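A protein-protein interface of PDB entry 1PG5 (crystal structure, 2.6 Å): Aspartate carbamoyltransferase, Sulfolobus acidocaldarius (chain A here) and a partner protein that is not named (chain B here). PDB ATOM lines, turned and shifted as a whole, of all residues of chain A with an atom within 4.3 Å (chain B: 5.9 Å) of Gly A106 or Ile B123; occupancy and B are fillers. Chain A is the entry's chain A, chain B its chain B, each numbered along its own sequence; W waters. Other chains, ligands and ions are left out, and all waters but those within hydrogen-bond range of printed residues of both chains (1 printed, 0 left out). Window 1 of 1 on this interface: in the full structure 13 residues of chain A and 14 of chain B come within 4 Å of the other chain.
OD2 of Asp B127 sits at hydrogen-bond distance from N of Leu A84, 3.0 Å away.
The side-chain amide oxygen (OD1) of Asn B126 lies within hydrogen-bond range of the side-chain hydroxyl (OH) of Tyr A104 (3.4 Å).
O of Tyr B121 is in hydrogen-bond range of N of Asp A105 (2.8 Å).
N of Ile B123 sits at hydrogen-bond distance from O of Asp A105, 2.9 Å away.
OD1 of Asp A105 sits at hydrogen-bond distance from N of His A127, at 3.2 Å.
The backbone NH (N) of Gly A106 sits at hydrogen-bond distance from the side-chain carboxylate (OD2) of Asp A124 (2.8 Å).
OD2 of Asp A124 is in hydrogen-bond range of ND1 of His A127 (2.6 Å).
OG1 of Thr B124 lies close to SG of Cys B122, 2.9 Å away.
The backbone carbonyl oxygen (O) of Cys B122 lies within hydrogen-bond range of the side-chain amide nitrogen (ND2) of Asn B126 (3.0 Å).
Among the printed residues, merely in contact across the chains: Tyr A104 with Tyr B121, Tyr A104 with Ile B123, Asp A105 with Cys B122, Asp A105 with Cys B149, Gly A106 with Ile B123, Gly A106 with Tyr B148, Arg A109 with Tyr B148, Phe A110 with Asp B127, Phe A110 with Ala B130, Phe A110 with Tyr B148 and His A127 with Tyr B148.
Hydrophobic or aromatic side chains of chain A that line the printed part of chain B: Leu A84, Tyr A104, Phe A110 and His A127.
Of the 11 printed residues of chain B, 8 touch a printed residue of chain A.
Hydrophobic or aromatic side chains of chain B within 4 Å of the printed part of chain A: Tyr B121, Ile B123, Ala B130 and Tyr B148.
Among the printed residues, no Asp or Glu carboxylate lies within 4 Å of a Lys or Arg side-chain nitrogen of the other chain.
Water W1 bridges N of Leu A84 (3.2 Å) and OD2 of Asp B127 (3.4 Å).
Gly A106 touches just these residues of chain B: Ile B123 (3.6 Å) and Tyr B148 (3.3 Å).
Of the printed residues of chain B, Arg A109 touches Tyr B148 (3.7 Å).
Of the printed residues of chain B, Asp A105 touches Tyr B121, Cys B122, Ile B123 and Cys B149.
Of the printed residues of chain B, Tyr A104 touches Tyr B121, Ile B123 and Asn B126.
Asp A124 touches none of the printed residues of chain B.
Ala A107 touches none of the printed residues of chain B.
The nearest residue of chain B that does not touch Gly A106 is Cys B149 (4.9 Å).
The nearest printed residue of chain B that does not touch Asp A105 is Tyr B148 (4.2 Å).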
ATOM      1  N   LEU A  84     -25.761 -12.942  22.605  1.00  0.00           N
ATOM      2  CA  LEU A  84     -25.469 -11.714  21.816  1.00  0.00           C
ATOM      3  C   LEU A  84     -26.779 -10.907  21.643  1.00  0.00           C
ATOM      4  O   LEU A  84     -26.769  -9.697  21.800  1.00  0.00           O
ATOM      5  CB  LEU A  84     -24.945 -12.038  20.443  1.00  0.00           C
ATOM      6  CG  LEU A  84     -24.069 -11.086  19.657  1.00  0.00           C
ATOM      7  CD1 LEU A  84     -24.251 -11.280  18.161  1.00  0.00           C
ATOM      8  CD2 LEU A  84     -24.087  -9.678  19.968  1.00  0.00           C
ATOM      9  N   TYR A 104     -17.342 -14.632  16.658  1.00  0.00           N
ATOM     10  CA  TYR A 104     -18.141 -15.546  15.844  1.00  0.00           C
ATOM     11  C   TYR A 104     -18.477 -14.940  14.489  1.00  0.00           C
ATOM     12  O   TYR A 104     -18.824 -13.814  14.396  1.00  0.00           O
ATOM     13  CB  TYR A 104     -19.355 -16.023  16.623  1.00  0.00           C
ATOM     14  CG  TYR A 104     -19.043 -16.941  17.793  1.00  0.00           C
ATOM     15  CD1 TYR A 104     -17.972 -17.848  17.787  1.00  0.00           C
ATOM     16  CD2 TYR A 104     -19.793 -16.879  18.921  1.00  0.00           C
ATOM     17  CE1 TYR A 104     -17.699 -18.631  18.901  1.00  0.00           C
ATOM     18  CE2 TYR A 104     -19.546 -17.679  20.027  1.00  0.00           C
ATOM     19  CZ  TYR A 104     -18.509 -18.540  20.031  1.00  0.00           C
ATOM     20  OH  TYR A 104     -18.347 -19.271  21.207  1.00  0.00           O
ATOM     21  N   ASP A 105     -18.238 -15.673  13.401  1.00  0.00           N
ATOM     22  CA  ASP A 105     -18.572 -15.219  12.044  1.00  0.00           C
ATOM     23  C   ASP A 105     -20.057 -14.915  11.969  1.00  0.00           C
ATOM     24  O   ASP A 105     -20.852 -15.701  12.403  1.00  0.00           O
ATOM     25  CB  ASP A 105     -18.306 -16.343  11.030  1.00  0.00           C
ATOM     26  CG  ASP A 105     -16.869 -16.830  11.065  1.00  0.00           C
ATOM     27  OD1 ASP A 105     -16.005 -15.997  10.848  1.00  0.00           O
ATOM     28  OD2 ASP A 105     -16.506 -17.997  11.320  1.00  0.00           O
ATOM     29  N   GLY A 106     -20.432 -13.774  11.425  1.00  0.00           N
ATOM     30  CA  GLY A 106     -21.846 -13.513  11.190  1.00  0.00           C
ATOM     31  C   GLY A 106     -22.424 -12.798  12.366  1.00  0.00           C
ATOM     32  O   GLY A 106     -23.586 -12.423  12.338  1.00  0.00           O
ATOM     33  N   ALA A 107     -21.610 -12.515  13.388  1.00  0.00           N
ATOM     34  CA  ALA A 107     -22.186 -11.931  14.584  1.00  0.00           C
ATOM     35  C   ALA A 107     -22.822 -10.595  14.328  1.00  0.00           C
ATOM     36  O   ALA A 107     -23.846 -10.302  14.901  1.00  0.00           O
ATOM     37  CB  ALA A 107     -21.182 -11.789  15.640  1.00  0.00           C
ATOM     38  N   SER A 108     -22.186  -9.784  13.511  1.00  0.00           N
ATOM     39  CA  SER A 108     -22.666  -8.437  13.245  1.00  0.00           C
ATOM     40  C   SER A 108     -23.899  -8.466  12.385  1.00  0.00           C
ATOM     41  O   SER A 108     -24.786  -7.598  12.549  1.00  0.00           O
ATOM     42  CB  SER A 108     -21.644  -7.647  12.416  1.00  0.00           C
ATOM     43  OG  SER A 108     -20.699  -7.152  13.334  1.00  0.00           O
ATOM     44  N   ARG A 109     -23.866  -9.361  11.384  1.00  0.00           N
ATOM     45  CA  ARG A 109     -25.055  -9.601  10.603  1.00  0.00           C
ATOM     46  C   ARG A 109     -26.249  -9.889  11.508  1.00  0.00           C
ATOM     47  O   ARG A 109     -27.279  -9.215  11.399  1.00  0.00           O
ATOM     48  CB  ARG A 109     -24.913 -10.729   9.646  1.00  0.00           C
ATOM     49  CG  ARG A 109     -25.982 -10.682   8.585  1.00  0.00           C
ATOM     50  CD  ARG A 109     -26.183 -11.961   7.800  1.00  0.00           C
ATOM     51  NE  ARG A 109     -26.483 -11.608   6.438  1.00  0.00           N
ATOM     52  CZ  ARG A 109     -27.572 -11.960   5.730  1.00  0.00           C
ATOM     53  NH1 ARG A 109     -28.572 -12.667   6.225  1.00  0.00           N
ATOM     54  NH2 ARG A 109     -27.671 -11.529   4.485  1.00  0.00           N
ATOM     55  N   PHE A 110     -26.080 -10.824  12.430  1.00  0.00           N
ATOM     56  CA  PHE A 110     -27.146 -11.157  13.311  1.00  0.00           C
ATOM     57  C   PHE A 110     -27.517  -9.962  14.207  1.00  0.00           C
ATOM     58  O   PHE A 110     -28.695  -9.669  14.408  1.00  0.00           O
ATOM     59  CB  PHE A 110     -26.777 -12.408  14.107  1.00  0.00           C
ATOM     60  CG  PHE A 110     -27.744 -12.761  15.210  1.00  0.00           C
ATOM     61  CD1 PHE A 110     -27.348 -12.705  16.501  1.00  0.00           C
ATOM     62  CD2 PHE A 110     -29.045 -13.121  14.922  1.00  0.00           C
ATOM     63  CE1 PHE A 110     -28.216 -13.011  17.546  1.00  0.00           C
ATOM     64  CE2 PHE A 110     -29.971 -13.402  15.937  1.00  0.00           C
ATOM     65  CZ  PHE A 110     -29.555 -13.380  17.260  1.00  0.00           C
ATOM     66  N   ASP A 124     -15.755  -9.575  12.586  1.00  0.00           N
ATOM     67  CA  ASP A 124     -16.494 -10.709  13.115  1.00  0.00           C
ATOM     68  C   ASP A 124     -15.751 -12.016  12.759  1.00  0.00           C
ATOM     69  O   ASP A 124     -15.645 -12.393  11.619  1.00  0.00           O
ATOM     70  CB  ASP A 124     -17.937 -10.623  12.598  1.00  0.00           C
ATOM     71  CG  ASP A 124     -18.071 -10.809  11.035  1.00  0.00           C
ATOM     72  OD1 ASP A 124     -17.261 -10.211  10.225  1.00  0.00           O
ATOM     73  OD2 ASP A 124     -18.997 -11.569  10.566  1.00  0.00           O
ATOM     74  N   HIS A 127     -14.508 -13.650   9.280  1.00  0.00           N
ATOM     75  CA  HIS A 127     -15.344 -13.365   8.125  1.00  0.00           C
ATOM     76  C   HIS A 127     -15.001 -12.018   7.433  1.00  0.00           C
ATOM     77  O   HIS A 127     -14.406 -12.064   6.348  1.00  0.00           O
ATOM     78  CB  HIS A 127     -16.776 -13.560   8.586  1.00  0.00           C
ATOM     79  CG  HIS A 127     -17.801 -13.076   7.637  1.00  0.00           C
ATOM     80  ND1 HIS A 127     -18.677 -12.066   7.988  1.00  0.00           N
ATOM     81  CD2 HIS A 127     -18.123 -13.466   6.384  1.00  0.00           C
ATOM     82  CE1 HIS A 127     -19.472 -11.826   6.965  1.00  0.00           C
ATOM     83  NE2 HIS A 127     -19.170 -12.675   5.990  1.00  0.00           N
ATOM     84  N   TYR B 121     -17.710 -21.830  14.629  1.00  0.00           N
ATOM     85  CA  TYR B 121     -17.510 -20.405  14.976  1.00  0.00           C
ATOM     86  C   TYR B 121     -18.536 -19.539  14.308  1.00  0.00           C
ATOM     87  O   TYR B 121     -18.435 -18.348  14.355  1.00  0.00           O
ATOM     88  CB  TYR B 121     -16.115 -19.928  14.592  1.00  0.00           C
ATOM     89  CG  TYR B 121     -15.031 -20.533  15.446  1.00  0.00           C
ATOM     90  CD1 TYR B 121     -14.253 -21.584  14.958  1.00  0.00           C
ATOM     91  CD2 TYR B 121     -14.745 -20.034  16.739  1.00  0.00           C
ATOM     92  CE1 TYR B 121     -13.255 -22.132  15.707  1.00  0.00           C
ATOM     93  CE2 TYR B 121     -13.732 -20.589  17.500  1.00  0.00           C
ATOM     94  CZ  TYR B 121     -13.019 -21.670  16.960  1.00  0.00           C
ATOM     95  OH  TYR B 121     -12.021 -22.273  17.632  1.00  0.00           O
ATOM     96  N   CYS B 122     -19.555 -20.116  13.697  1.00  0.00           N
ATOM     97  CA  CYS B 122     -20.629 -19.318  13.107  1.00  0.00           C
ATOM     98  C   CYS B 122     -21.525 -18.919  14.216  1.00  0.00           C
ATOM     99  O   CYS B 122     -21.789 -19.766  15.044  1.00  0.00           O
ATOM    100  CB  CYS B 122     -21.386 -20.181  12.112  1.00  0.00           C
ATOM    101  SG  CYS B 122     -22.776 -19.404  11.288  1.00  0.00           S
ATOM    102  N   ILE B 123     -21.981 -17.661  14.246  1.00  0.00           N
ATOM    103  CA  ILE B 123     -22.954 -17.205  15.213  1.00  0.00           C
ATOM    104  C   ILE B 123     -24.166 -18.137  15.337  1.00  0.00           C
ATOM    105  O   ILE B 123     -24.622 -18.352  16.450  1.00  0.00           O
ATOM    106  CB  ILE B 123     -23.396 -15.806  14.905  1.00  0.00           C
ATOM    107  CG1 ILE B 123     -24.089 -15.165  16.121  1.00  0.00           C
ATOM    108  CG2 ILE B 123     -24.247 -15.749  13.604  1.00  0.00           C
ATOM    109  CD1 ILE B 123     -23.183 -15.057  17.328  1.00  0.00           C
ATOM    110  N   THR B 124     -24.658 -18.726  14.237  1.00  0.00           N
ATOM    111  CA  THR B 124     -25.763 -19.714  14.297  1.00  0.00           C
ATOM    112  C   THR B 124     -25.489 -21.037  15.057  1.00  0.00           C
ATOM    113  O   THR B 124     -26.422 -21.734  15.485  1.00  0.00           O
ATOM    114  CB  THR B 124     -26.308 -20.004  12.901  1.00  0.00           C
ATOM    115  OG1 THR B 124     -25.333 -20.647  12.054  1.00  0.00           O
ATOM    116  CG2 THR B 124     -26.538 -18.632  12.201  1.00  0.00           C
ATOM    117  N   SER B 125     -24.216 -21.352  15.259  1.00  0.00           N
ATOM    118  CA  SER B 125     -23.773 -22.566  15.972  1.00  0.00           C
ATOM    119  C   SER B 125     -23.557 -22.178  17.402  1.00  0.00           C
ATOM    120  O   SER B 125     -23.172 -23.005  18.138  1.00  0.00           O
ATOM    121  CB  SER B 125     -22.441 -23.095  15.430  1.00  0.00           C
ATOM    122  OG  SER B 125     -22.558 -23.561  14.073  1.00  0.00           O
ATOM    123  N   ASN B 126     -23.805 -20.935  17.811  1.00  0.00           N
ATOM    124  CA  ASN B 126     -23.557 -20.540  19.190  1.00  0.00           C
ATOM    125  C   ASN B 126     -24.678 -19.783  19.955  1.00  0.00           C
ATOM    126  O   ASN B 126     -24.745 -19.880  21.148  1.00  0.00           O
ATOM    127  CB  ASN B 126     -22.240 -19.735  19.225  1.00  0.00           C
ATOM    128  CG  ASN B 126     -21.051 -20.589  18.869  1.00  0.00           C
ATOM    129  OD1 ASN B 126     -20.611 -21.300  19.712  1.00  0.00           O
ATOM    130  ND2 ASN B 126     -20.553 -20.543  17.621  1.00  0.00           N
ATOM    131  N   ASP B 127     -25.531 -19.027  19.292  1.00  0.00           N
ATOM    132  CA  ASP B 127     -26.561 -18.215  19.906  1.00  0.00           C
ATOM    133  C   ASP B 127     -27.862 -18.917  19.527  1.00  0.00           C
ATOM    134  O   ASP B 127     -28.155 -19.091  18.338  1.00  0.00           O
ATOM    135  CB  ASP B 127     -26.515 -16.763  19.351  1.00  0.00           C
ATOM    136  CG  ASP B 127     -27.485 -15.754  20.101  1.00  0.00           C
ATOM    137  OD1 ASP B 127     -28.728 -15.972  20.258  1.00  0.00           O
ATOM    138  OD2 ASP B 127     -27.048 -14.669  20.551  1.00  0.00           O
ATOM    139  N   VAL B 128     -28.627 -19.335  20.525  1.00  0.00           N
ATOM    140  CA  VAL B 128     -29.933 -19.903  20.275  1.00  0.00           C
ATOM    141  C   VAL B 128     -30.897 -19.054  19.480  1.00  0.00           C
ATOM    142  O   VAL B 128     -31.760 -19.627  18.848  1.00  0.00           O
ATOM    143  CB  VAL B 128     -30.730 -20.279  21.571  1.00  0.00           C
ATOM    144  CG1 VAL B 128     -30.409 -21.657  21.921  1.00  0.00           C
ATOM    145  CG2 VAL B 128     -30.463 -19.297  22.748  1.00  0.00           C
ATOM    146  N   ALA B 130     -30.104 -17.162  17.102  1.00  0.00           N
ATOM    147  CA  ALA B 130     -29.531 -16.997  15.791  1.00  0.00           C
ATOM    148  C   ALA B 130     -29.825 -18.239  14.951  1.00  0.00           C
ATOM    149  O   ALA B 130     -29.076 -19.161  14.895  1.00  0.00           O
ATOM    150  CB  ALA B 130     -28.005 -16.779  15.952  1.00  0.00           C
ATOM    151  N   TYR B 148     -24.693 -16.248   7.250  1.00  0.00           N
ATOM    152  CA  TYR B 148     -23.878 -15.566   8.231  1.00  0.00           C
ATOM    153  C   TYR B 148     -22.387 -15.653   7.970  1.00  0.00           C
ATOM    154  O   TYR B 148     -21.672 -14.672   8.057  1.00  0.00           O
ATOM    155  CB  TYR B 148     -24.253 -16.155   9.584  1.00  0.00           C
ATOM    156  CG  TYR B 148     -25.627 -15.727   9.894  1.00  0.00           C
ATOM    157  CD1 TYR B 148     -25.869 -14.465  10.466  1.00  0.00           C
ATOM    158  CD2 TYR B 148     -26.710 -16.510   9.555  1.00  0.00           C
ATOM    159  CE1 TYR B 148     -27.168 -14.047  10.788  1.00  0.00           C
ATOM    160  CE2 TYR B 148     -28.044 -16.078   9.844  1.00  0.00           C
ATOM    161  CZ  TYR B 148     -28.242 -14.840  10.440  1.00  0.00           C
ATOM    162  OH  TYR B 148     -29.523 -14.416  10.708  1.00  0.00           O
ATOM    163  N   CYS B 149     -21.920 -16.848   7.625  1.00  0.00           N
ATOM    164  CA  CYS B 149     -20.491 -17.109   7.451  1.00  0.00           C
ATOM    165  C   CYS B 149     -20.038 -17.625   6.088  1.00  0.00           C
ATOM    166  O   CYS B 149     -18.874 -17.847   5.907  1.00  0.00           O
ATOM    167  CB  CYS B 149     -20.040 -18.100   8.517  1.00  0.00           C
ATOM    168  SG  CYS B 149     -20.516 -19.800   8.258  1.00  0.00           S
HETATM  169  O   HOH W   1     -23.980 -15.508  21.728  1.00  0.00           O
